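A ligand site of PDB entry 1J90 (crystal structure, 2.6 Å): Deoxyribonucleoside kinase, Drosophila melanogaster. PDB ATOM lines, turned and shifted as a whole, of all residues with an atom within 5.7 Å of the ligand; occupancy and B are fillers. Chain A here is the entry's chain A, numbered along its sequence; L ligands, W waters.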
ATOM      1  N   ILE A  29       8.374  23.012 -25.748  1.00  0.00           N
ATOM      2  CA  ILE A  29       9.787  22.714 -25.864  1.00  0.00           C
ATOM      3  C   ILE A  29      10.060  22.541 -27.360  1.00  0.00           C
ATOM      4  O   ILE A  29       9.362  21.798 -28.038  1.00  0.00           O
ATOM      5  CB  ILE A  29      10.134  21.406 -25.133  1.00  0.00           C
ATOM      6  CG1 ILE A  29       9.539  21.397 -23.725  1.00  0.00           C
ATOM      7  CG2 ILE A  29      11.635  21.208 -25.098  1.00  0.00           C
ATOM      8  CD1 ILE A  29       9.695  20.043 -23.024  1.00  0.00           C
ATOM      9  N   GLU A  52      15.688  31.834 -20.052  1.00  0.00           N
ATOM     10  CA  GLU A  52      15.354  30.808 -19.080  1.00  0.00           C
ATOM     11  C   GLU A  52      16.622  30.415 -18.334  1.00  0.00           C
ATOM     12  O   GLU A  52      17.656  30.163 -18.946  1.00  0.00           O
ATOM     13  CB  GLU A  52      14.749  29.568 -19.750  1.00  0.00           C
ATOM     14  CG  GLU A  52      13.243  29.453 -19.631  1.00  0.00           C
ATOM     15  CD  GLU A  52      12.727  28.091 -20.072  1.00  0.00           C
ATOM     16  OE1 GLU A  52      13.257  27.533 -21.048  1.00  0.00           O
ATOM     17  OE2 GLU A  52      11.787  27.582 -19.423  1.00  0.00           O
ATOM     18  N   VAL A  54      17.944  27.925 -17.444  1.00  0.00           N
ATOM     19  CA  VAL A  54      18.198  26.496 -17.611  1.00  0.00           C
ATOM     20  C   VAL A  54      19.559  26.029 -17.081  1.00  0.00           C
ATOM     21  O   VAL A  54      19.650  24.966 -16.474  1.00  0.00           O
ATOM     22  CB  VAL A  54      18.061  26.068 -19.091  1.00  0.00           C
ATOM     23  CG1 VAL A  54      19.100  26.767 -19.945  1.00  0.00           C
ATOM     24  CG2 VAL A  54      18.210  24.556 -19.217  1.00  0.00           C
ATOM     25  N   TRP A  57      19.423  25.311 -13.546  1.00  0.00           N
ATOM     26  CA  TRP A  57      18.747  24.050 -13.320  1.00  0.00           C
ATOM     27  C   TRP A  57      19.716  22.881 -13.499  1.00  0.00           C
ATOM     28  O   TRP A  57      19.563  21.812 -12.896  1.00  0.00           O
ATOM     29  CB  TRP A  57      17.552  23.889 -14.274  1.00  0.00           C
ATOM     30  CG  TRP A  57      16.559  25.032 -14.220  1.00  0.00           C
ATOM     31  CD1 TRP A  57      16.425  25.972 -13.232  1.00  0.00           C
ATOM     32  CD2 TRP A  57      15.565  25.363 -15.200  1.00  0.00           C
ATOM     33  NE1 TRP A  57      15.421  26.854 -13.540  1.00  0.00           N
ATOM     34  CE2 TRP A  57      14.872  26.502 -14.741  1.00  0.00           C
ATOM     35  CE3 TRP A  57      15.195  24.801 -16.432  1.00  0.00           C
ATOM     36  CZ2 TRP A  57      13.833  27.092 -15.475  1.00  0.00           C
ATOM     37  CZ3 TRP A  57      14.168  25.391 -17.157  1.00  0.00           C
ATOM     38  CH2 TRP A  57      13.491  26.523 -16.661  1.00  0.00           C
ATOM     39  N   LEU A  66      17.563  19.222 -13.861  1.00  0.00           N
ATOM     40  CA  LEU A  66      16.922  19.012 -15.143  1.00  0.00           C
ATOM     41  C   LEU A  66      17.063  17.557 -15.576  1.00  0.00           C
ATOM     42  O   LEU A  66      16.093  16.916 -15.971  1.00  0.00           O
ATOM     43  CB  LEU A  66      17.513  19.934 -16.209  1.00  0.00           C
ATOM     44  CG  LEU A  66      16.867  19.879 -17.593  1.00  0.00           C
ATOM     45  CD1 LEU A  66      15.396  20.278 -17.499  1.00  0.00           C
ATOM     46  CD2 LEU A  66      17.604  20.763 -18.598  1.00  0.00           C
ATOM     47  N   MET A  69      15.087  15.182 -13.318  1.00  0.00           N
ATOM     48  CA  MET A  69      13.653  15.281 -13.570  1.00  0.00           C
ATOM     49  C   MET A  69      13.240  14.379 -14.730  1.00  0.00           C
ATOM     50  O   MET A  69      12.287  13.604 -14.608  1.00  0.00           O
ATOM     51  CB  MET A  69      13.247  16.727 -13.840  1.00  0.00           C
ATOM     52  CG  MET A  69      11.775  16.888 -14.156  1.00  0.00           C
ATOM     53  SD  MET A  69      11.443  16.586 -15.889  1.00  0.00           S
ATOM     54  CE  MET A  69      12.205  18.034 -16.639  1.00  0.00           C
ATOM     55  N   TYR A  70      13.956  14.460 -15.843  1.00  0.00           N
ATOM     56  CA  TYR A  70      13.633  13.639 -17.001  1.00  0.00           C
ATOM     57  C   TYR A  70      13.924  12.170 -16.780  1.00  0.00           C
ATOM     58  O   TYR A  70      13.305  11.298 -17.393  1.00  0.00           O
ATOM     59  CB  TYR A  70      14.384  14.142 -18.231  1.00  0.00           C
ATOM     60  CG  TYR A  70      13.678  15.280 -18.938  1.00  0.00           C
ATOM     61  CD1 TYR A  70      14.354  16.448 -19.255  1.00  0.00           C
ATOM     62  CD2 TYR A  70      12.333  15.172 -19.278  1.00  0.00           C
ATOM     63  CE1 TYR A  70      13.711  17.487 -19.900  1.00  0.00           C
ATOM     64  CE2 TYR A  70      11.680  16.209 -19.921  1.00  0.00           C
ATOM     65  CZ  TYR A  70      12.372  17.355 -20.225  1.00  0.00           C
ATOM     66  OH  TYR A  70      11.732  18.390 -20.850  1.00  0.00           O
ATOM     67  N   PHE A  80      12.420  19.825  -8.858  1.00  0.00           N
ATOM     68  CA  PHE A  80      12.752  20.566 -10.074  1.00  0.00           C
ATOM     69  C   PHE A  80      11.820  21.745 -10.292  1.00  0.00           C
ATOM     70  O   PHE A  80      12.271  22.886 -10.422  1.00  0.00           O
ATOM     71  CB  PHE A  80      12.701  19.636 -11.299  1.00  0.00           C
ATOM     72  CG  PHE A  80      12.933  20.345 -12.608  1.00  0.00           C
ATOM     73  CD1 PHE A  80      14.199  20.792 -12.951  1.00  0.00           C
ATOM     74  CD2 PHE A  80      11.887  20.566 -13.488  1.00  0.00           C
ATOM     75  CE1 PHE A  80      14.422  21.455 -14.155  1.00  0.00           C
ATOM     76  CE2 PHE A  80      12.102  21.208 -14.695  1.00  0.00           C
ATOM     77  CZ  PHE A  80      13.369  21.653 -15.028  1.00  0.00           C
ATOM     78  N   GLN A  81      10.520  21.479 -10.320  1.00  0.00           N
ATOM     79  CA  GLN A  81       9.534  22.538 -10.532  1.00  0.00           C
ATOM     80  C   GLN A  81       9.588  23.601  -9.446  1.00  0.00           C
ATOM     81  O   GLN A  81       9.363  24.788  -9.705  1.00  0.00           O
ATOM     82  CB  GLN A  81       8.125  21.958 -10.637  1.00  0.00           C
ATOM     83  CG  GLN A  81       7.872  21.174 -11.923  1.00  0.00           C
ATOM     84  CD  GLN A  81       8.073  22.019 -13.169  1.00  0.00           C
ATOM     85  OE1 GLN A  81       8.016  23.248 -13.116  1.00  0.00           O
ATOM     86  NE2 GLN A  81       8.304  21.347 -14.294  1.00  0.00           N
ATOM     87  N   VAL A  84      12.376  25.716 -10.256  1.00  0.00           N
ATOM     88  CA  VAL A  84      11.966  26.512 -11.402  1.00  0.00           C
ATOM     89  C   VAL A  84      11.177  27.713 -10.905  1.00  0.00           C
ATOM     90  O   VAL A  84      11.478  28.845 -11.251  1.00  0.00           O
ATOM     91  CB  VAL A  84      11.121  25.702 -12.411  1.00  0.00           C
ATOM     92  CG1 VAL A  84      10.504  26.606 -13.459  1.00  0.00           C
ATOM     93  CG2 VAL A  84      11.972  24.625 -13.069  1.00  0.00           C
ATOM     94  N   ARG A 105       9.592  32.516 -20.861  1.00  0.00           N
ATOM     95  CA  ARG A 105       8.824  31.707 -19.929  1.00  0.00           C
ATOM     96  C   ARG A 105       8.522  32.497 -18.675  1.00  0.00           C
ATOM     97  O   ARG A 105       8.993  33.627 -18.512  1.00  0.00           O
ATOM     98  CB  ARG A 105       9.553  30.417 -19.597  1.00  0.00           C
ATOM     99  CG  ARG A 105       9.586  29.453 -20.760  1.00  0.00           C
ATOM    100  CD  ARG A 105       8.411  28.522 -20.789  1.00  0.00           C
ATOM    101  NE  ARG A 105       8.465  27.593 -21.917  1.00  0.00           N
ATOM    102  CZ  ARG A 105       9.302  26.583 -22.000  1.00  0.00           C
ATOM    103  NH1 ARG A 105      10.168  26.361 -21.019  1.00  0.00           N
ATOM    104  NH2 ARG A 105       9.294  25.787 -23.060  1.00  0.00           N
ATOM    105  N   SER A 109       3.604  29.683 -17.019  1.00  0.00           N
ATOM    106  CA  SER A 109       3.692  28.528 -17.899  1.00  0.00           C
ATOM    107  C   SER A 109       4.098  27.320 -17.074  1.00  0.00           C
ATOM    108  O   SER A 109       3.673  26.198 -17.346  1.00  0.00           O
ATOM    109  CB  SER A 109       4.653  28.764 -19.072  1.00  0.00           C
ATOM    110  OG  SER A 109       5.932  29.196 -18.645  1.00  0.00           O
ATOM    111  N   ALA A 110       4.915  27.557 -16.053  1.00  0.00           N
ATOM    112  CA  ALA A 110       5.359  26.485 -15.176  1.00  0.00           C
ATOM    113  C   ALA A 110       4.180  25.910 -14.398  1.00  0.00           C
ATOM    114  O   ALA A 110       4.022  24.695 -14.299  1.00  0.00           O
ATOM    115  CB  ALA A 110       6.414  26.999 -14.210  1.00  0.00           C
ATOM    116  N   PHE A 114       3.600  22.981 -17.379  1.00  0.00           N
ATOM    117  CA  PHE A 114       4.514  21.933 -16.925  1.00  0.00           C
ATOM    118  C   PHE A 114       4.118  21.194 -15.657  1.00  0.00           C
ATOM    119  O   PHE A 114       4.210  19.974 -15.590  1.00  0.00           O
ATOM    120  CB  PHE A 114       5.936  22.486 -16.828  1.00  0.00           C
ATOM    121  CG  PHE A 114       6.470  23.011 -18.131  1.00  0.00           C
ATOM    122  CD1 PHE A 114       6.201  24.297 -18.539  1.00  0.00           C
ATOM    123  CD2 PHE A 114       7.232  22.197 -18.948  1.00  0.00           C
ATOM    124  CE1 PHE A 114       6.676  24.770 -19.729  1.00  0.00           C
ATOM    125  CE2 PHE A 114       7.716  22.673 -20.150  1.00  0.00           C
ATOM    126  CZ  PHE A 114       7.438  23.956 -20.546  1.00  0.00           C
ATOM    127  N   VAL A 115       3.681  21.927 -14.631  1.00  0.00           N
ATOM    128  CA  VAL A 115       3.259  21.264 -13.395  1.00  0.00           C
ATOM    129  C   VAL A 115       1.971  20.485 -13.653  1.00  0.00           C
ATOM    130  O   VAL A 115       1.837  19.341 -13.213  1.00  0.00           O
ATOM    131  CB  VAL A 115       3.059  22.261 -12.229  1.00  0.00           C
ATOM    132  CG1 VAL A 115       2.182  21.650 -11.135  1.00  0.00           C
ATOM    133  CG2 VAL A 115       4.399  22.688 -11.658  1.00  0.00           C
ATOM    134  N   ARG A 167      18.133  19.394 -31.933  1.00  0.00           N
ATOM    135  CA  ARG A 167      18.821  20.125 -30.883  1.00  0.00           C
ATOM    136  C   ARG A 167      19.715  19.126 -30.148  1.00  0.00           C
ATOM    137  O   ARG A 167      20.823  19.459 -29.734  1.00  0.00           O
ATOM    138  CB  ARG A 167      17.814  20.733 -29.913  1.00  0.00           C
ATOM    139  CG  ARG A 167      18.194  22.107 -29.406  1.00  0.00           C
ATOM    140  CD  ARG A 167      18.132  22.240 -27.902  1.00  0.00           C
ATOM    141  NE  ARG A 167      16.898  21.708 -27.343  1.00  0.00           N
ATOM    142  CZ  ARG A 167      15.778  22.403 -27.195  1.00  0.00           C
ATOM    143  NH1 ARG A 167      15.717  23.668 -27.589  1.00  0.00           N
ATOM    144  NH2 ARG A 167      14.710  21.831 -26.651  1.00  0.00           N
ATOM    145  N   ARG A 169      19.617  17.904 -27.249  1.00  0.00           N
ATOM    146  CA  ARG A 169      19.931  18.219 -25.861  1.00  0.00           C
ATOM    147  C   ARG A 169      19.962  16.951 -25.008  1.00  0.00           C
ATOM    148  O   ARG A 169      19.015  16.155 -25.016  1.00  0.00           O
ATOM    149  CB  ARG A 169      18.916  19.215 -25.297  1.00  0.00           C
ATOM    150  CG  ARG A 169      19.162  19.607 -23.872  1.00  0.00           C
ATOM    151  CD  ARG A 169      18.252  20.724 -23.383  1.00  0.00           C
ATOM    152  NE  ARG A 169      18.542  21.988 -24.051  1.00  0.00           N
ATOM    153  CZ  ARG A 169      17.755  23.051 -23.996  1.00  0.00           C
ATOM    154  NH1 ARG A 169      16.631  23.007 -23.305  1.00  0.00           N
ATOM    155  NH2 ARG A 169      18.101  24.159 -24.633  1.00  0.00           N
ATOM    156  N   GLU A 172      16.893  15.996 -22.697  1.00  0.00           N
ATOM    157  CA  GLU A 172      15.619  15.786 -23.379  1.00  0.00           C
ATOM    158  C   GLU A 172      15.666  14.587 -24.313  1.00  0.00           C
ATOM    159  O   GLU A 172      14.741  14.335 -25.091  1.00  0.00           O
ATOM    160  CB  GLU A 172      15.241  17.042 -24.168  1.00  0.00           C
ATOM    161  CG  GLU A 172      15.613  18.324 -23.440  1.00  0.00           C
ATOM    162  CD  GLU A 172      15.296  19.579 -24.239  1.00  0.00           C
ATOM    163  OE1 GLU A 172      15.417  19.559 -25.482  1.00  0.00           O
ATOM    164  OE2 GLU A 172      14.931  20.581 -23.603  1.00  0.00           O
ATOM    165  N   TYR A 179       4.530  13.392 -24.960  1.00  0.00           N
ATOM    166  CA  TYR A 179       4.847  14.361 -23.915  1.00  0.00           C
ATOM    167  C   TYR A 179       4.643  15.768 -24.464  1.00  0.00           C
ATOM    168  O   TYR A 179       3.999  16.603 -23.817  1.00  0.00           O
ATOM    169  CB  TYR A 179       6.290  14.168 -23.467  1.00  0.00           C
ATOM    170  CG  TYR A 179       6.705  14.974 -22.244  1.00  0.00           C
ATOM    171  CD1 TYR A 179       6.376  14.559 -20.962  1.00  0.00           C
ATOM    172  CD2 TYR A 179       7.457  16.133 -22.389  1.00  0.00           C
ATOM    173  CE1 TYR A 179       6.767  15.285 -19.855  1.00  0.00           C
ATOM    174  CE2 TYR A 179       7.858  16.860 -21.284  1.00  0.00           C
ATOM    175  CZ  TYR A 179       7.507  16.437 -20.021  1.00  0.00           C
ATOM    176  OH  TYR A 179       7.911  17.182 -18.943  1.00  0.00           O
HETATM  177  N1  LIG L   1      11.116  22.873 -18.287  1.00  0.00           N
HETATM  178  C1  LIG L   1      10.309  22.165 -17.463  1.00  0.00           C
HETATM  179  N2  LIG L   1       9.453  22.784 -16.649  1.00  0.00           N
HETATM  180  C2  LIG L   1       9.367  24.111 -16.634  1.00  0.00           C
HETATM  181  C3  LIG L   1      10.178  24.861 -17.461  1.00  0.00           C
HETATM  182  C4  LIG L   1      11.066  24.202 -18.308  1.00  0.00           C
HETATM  183  O1  LIG L   1      10.378  20.842 -17.454  1.00  0.00           O
HETATM  184  N3  LIG L   1       8.453  24.744 -15.777  1.00  0.00           N
HETATM  185  C5  LIG L   1      12.052  22.160 -19.143  1.00  0.00           C
HETATM  186  C6  LIG L   1      11.556  22.072 -20.579  1.00  0.00           C
HETATM  187  C7  LIG L   1      12.862  21.996 -21.334  1.00  0.00           C
HETATM  188  C8  LIG L   1      13.829  22.841 -20.514  1.00  0.00           C
HETATM  189  O2  LIG L   1      13.326  22.829 -19.184  1.00  0.00           O
HETATM  190  O3  LIG L   1      13.275  20.643 -21.295  1.00  0.00           O
HETATM  191  C9  LIG L   1      13.810  24.255 -21.040  1.00  0.00           C
HETATM  192  O4  LIG L   1      14.292  24.527 -22.252  1.00  0.00           O
HETATM  193  O   HOH W   1       8.162  27.632 -16.909  1.00  0.00           O
HETATM  194  O   HOH W   2       9.035  18.850 -15.997  1.00  0.00           O
HETATM  195  O   HOH W   3      12.526  24.636 -24.205  1.00  0.00           O
HETATM  196  O   HOH W   4       9.531  19.103 -19.478  1.00  0.00           O
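Water W4 lies within hydrogen-bond range of OH of Tyr 179 (2.6 Å), OH of Tyr 70 (2.7 Å) and O1 of the ligand (2.8 Å).
Water W2 lies within hydrogen-bond range of an oxygen (O1) of the ligand (2.8 Å), the side-chain amide nitrogen of Gln 81 (3.1 Å) and the side-chain sulfur of Met 69 (3.3 Å).
Water W1 lies within hydrogen-bond range of a nitrogen (N3) of the ligand, the side-chain hydroxyl of Ser 109 and the backbone NH of Ala 110.
Merely in contact with the ligand: Phe 114, Phe 80, Trp 57, Ala 110, Met 69, Arg 105, Val 84, Ile 29 and Leu 66.
Hydrophobic or aromatic side chains within 4 Å of the ligand: Ile 29, Trp 57, Leu 66, Met 69, Tyr 70, Phe 80, Val 84, Ala 110 and Phe 114.
14 residues have an atom within 4 Å of the ligand: Ile 29, Glu 52, Trp 57, Leu 66, Met 69, Tyr 70, Phe 80, Gln 81, Val 84, Arg 105, Ala 110, Phe 114, Arg 169 and Glu 172.
Along chain A the residues within 4 Å of the ligand span positions 29 to 172.
O3 of the ligand lies within hydrogen-bond range of OH of Tyr 70 (2.8 Å).
A nitrogen (N2) of the ligand lies within hydrogen-bond range of the side-chain amide nitrogen (NE2) of Gln 81 (3.0 Å).
OE1 of Glu 52 sits close to O4 of the ligand, at 3.4 Å.
The side-chain carboxylate (OE2) of Glu 172 sits at hydrogen-bond distance from an oxygen (O3) of the ligand, 2.8 Å away.
NH1 of Arg 169 lies within hydrogen-bond range of O4 of the ligand (3.0 Å).
The backbone carbonyl oxygen (O) of Trp 57 is in hydrogen-bond range of the backbone NH (N) of Leu 66 (3.4 Å).
The guanidinium group of Arg 169 is in salt-bridge range of the side-chain carboxylate of Glu 172 (3.0 Å).
The guanidinium group (NH2) of Arg 167 lies within salt-bridge range of the side-chain carboxylate (OE1) of Glu 172 (2.7 Å).
The backbone carbonyl oxygen (O) of Ala 110 lies within hydrogen-bond range of the backbone NH (N) of Val 115, 2.8 Å away.
OE2 of Glu 52 is in salt-bridge range of NH1 of Arg 105 (2.6 Å).
N of Phe 114 sits at hydrogen-bond distance from O of Ser 109, at 3.2 Å.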
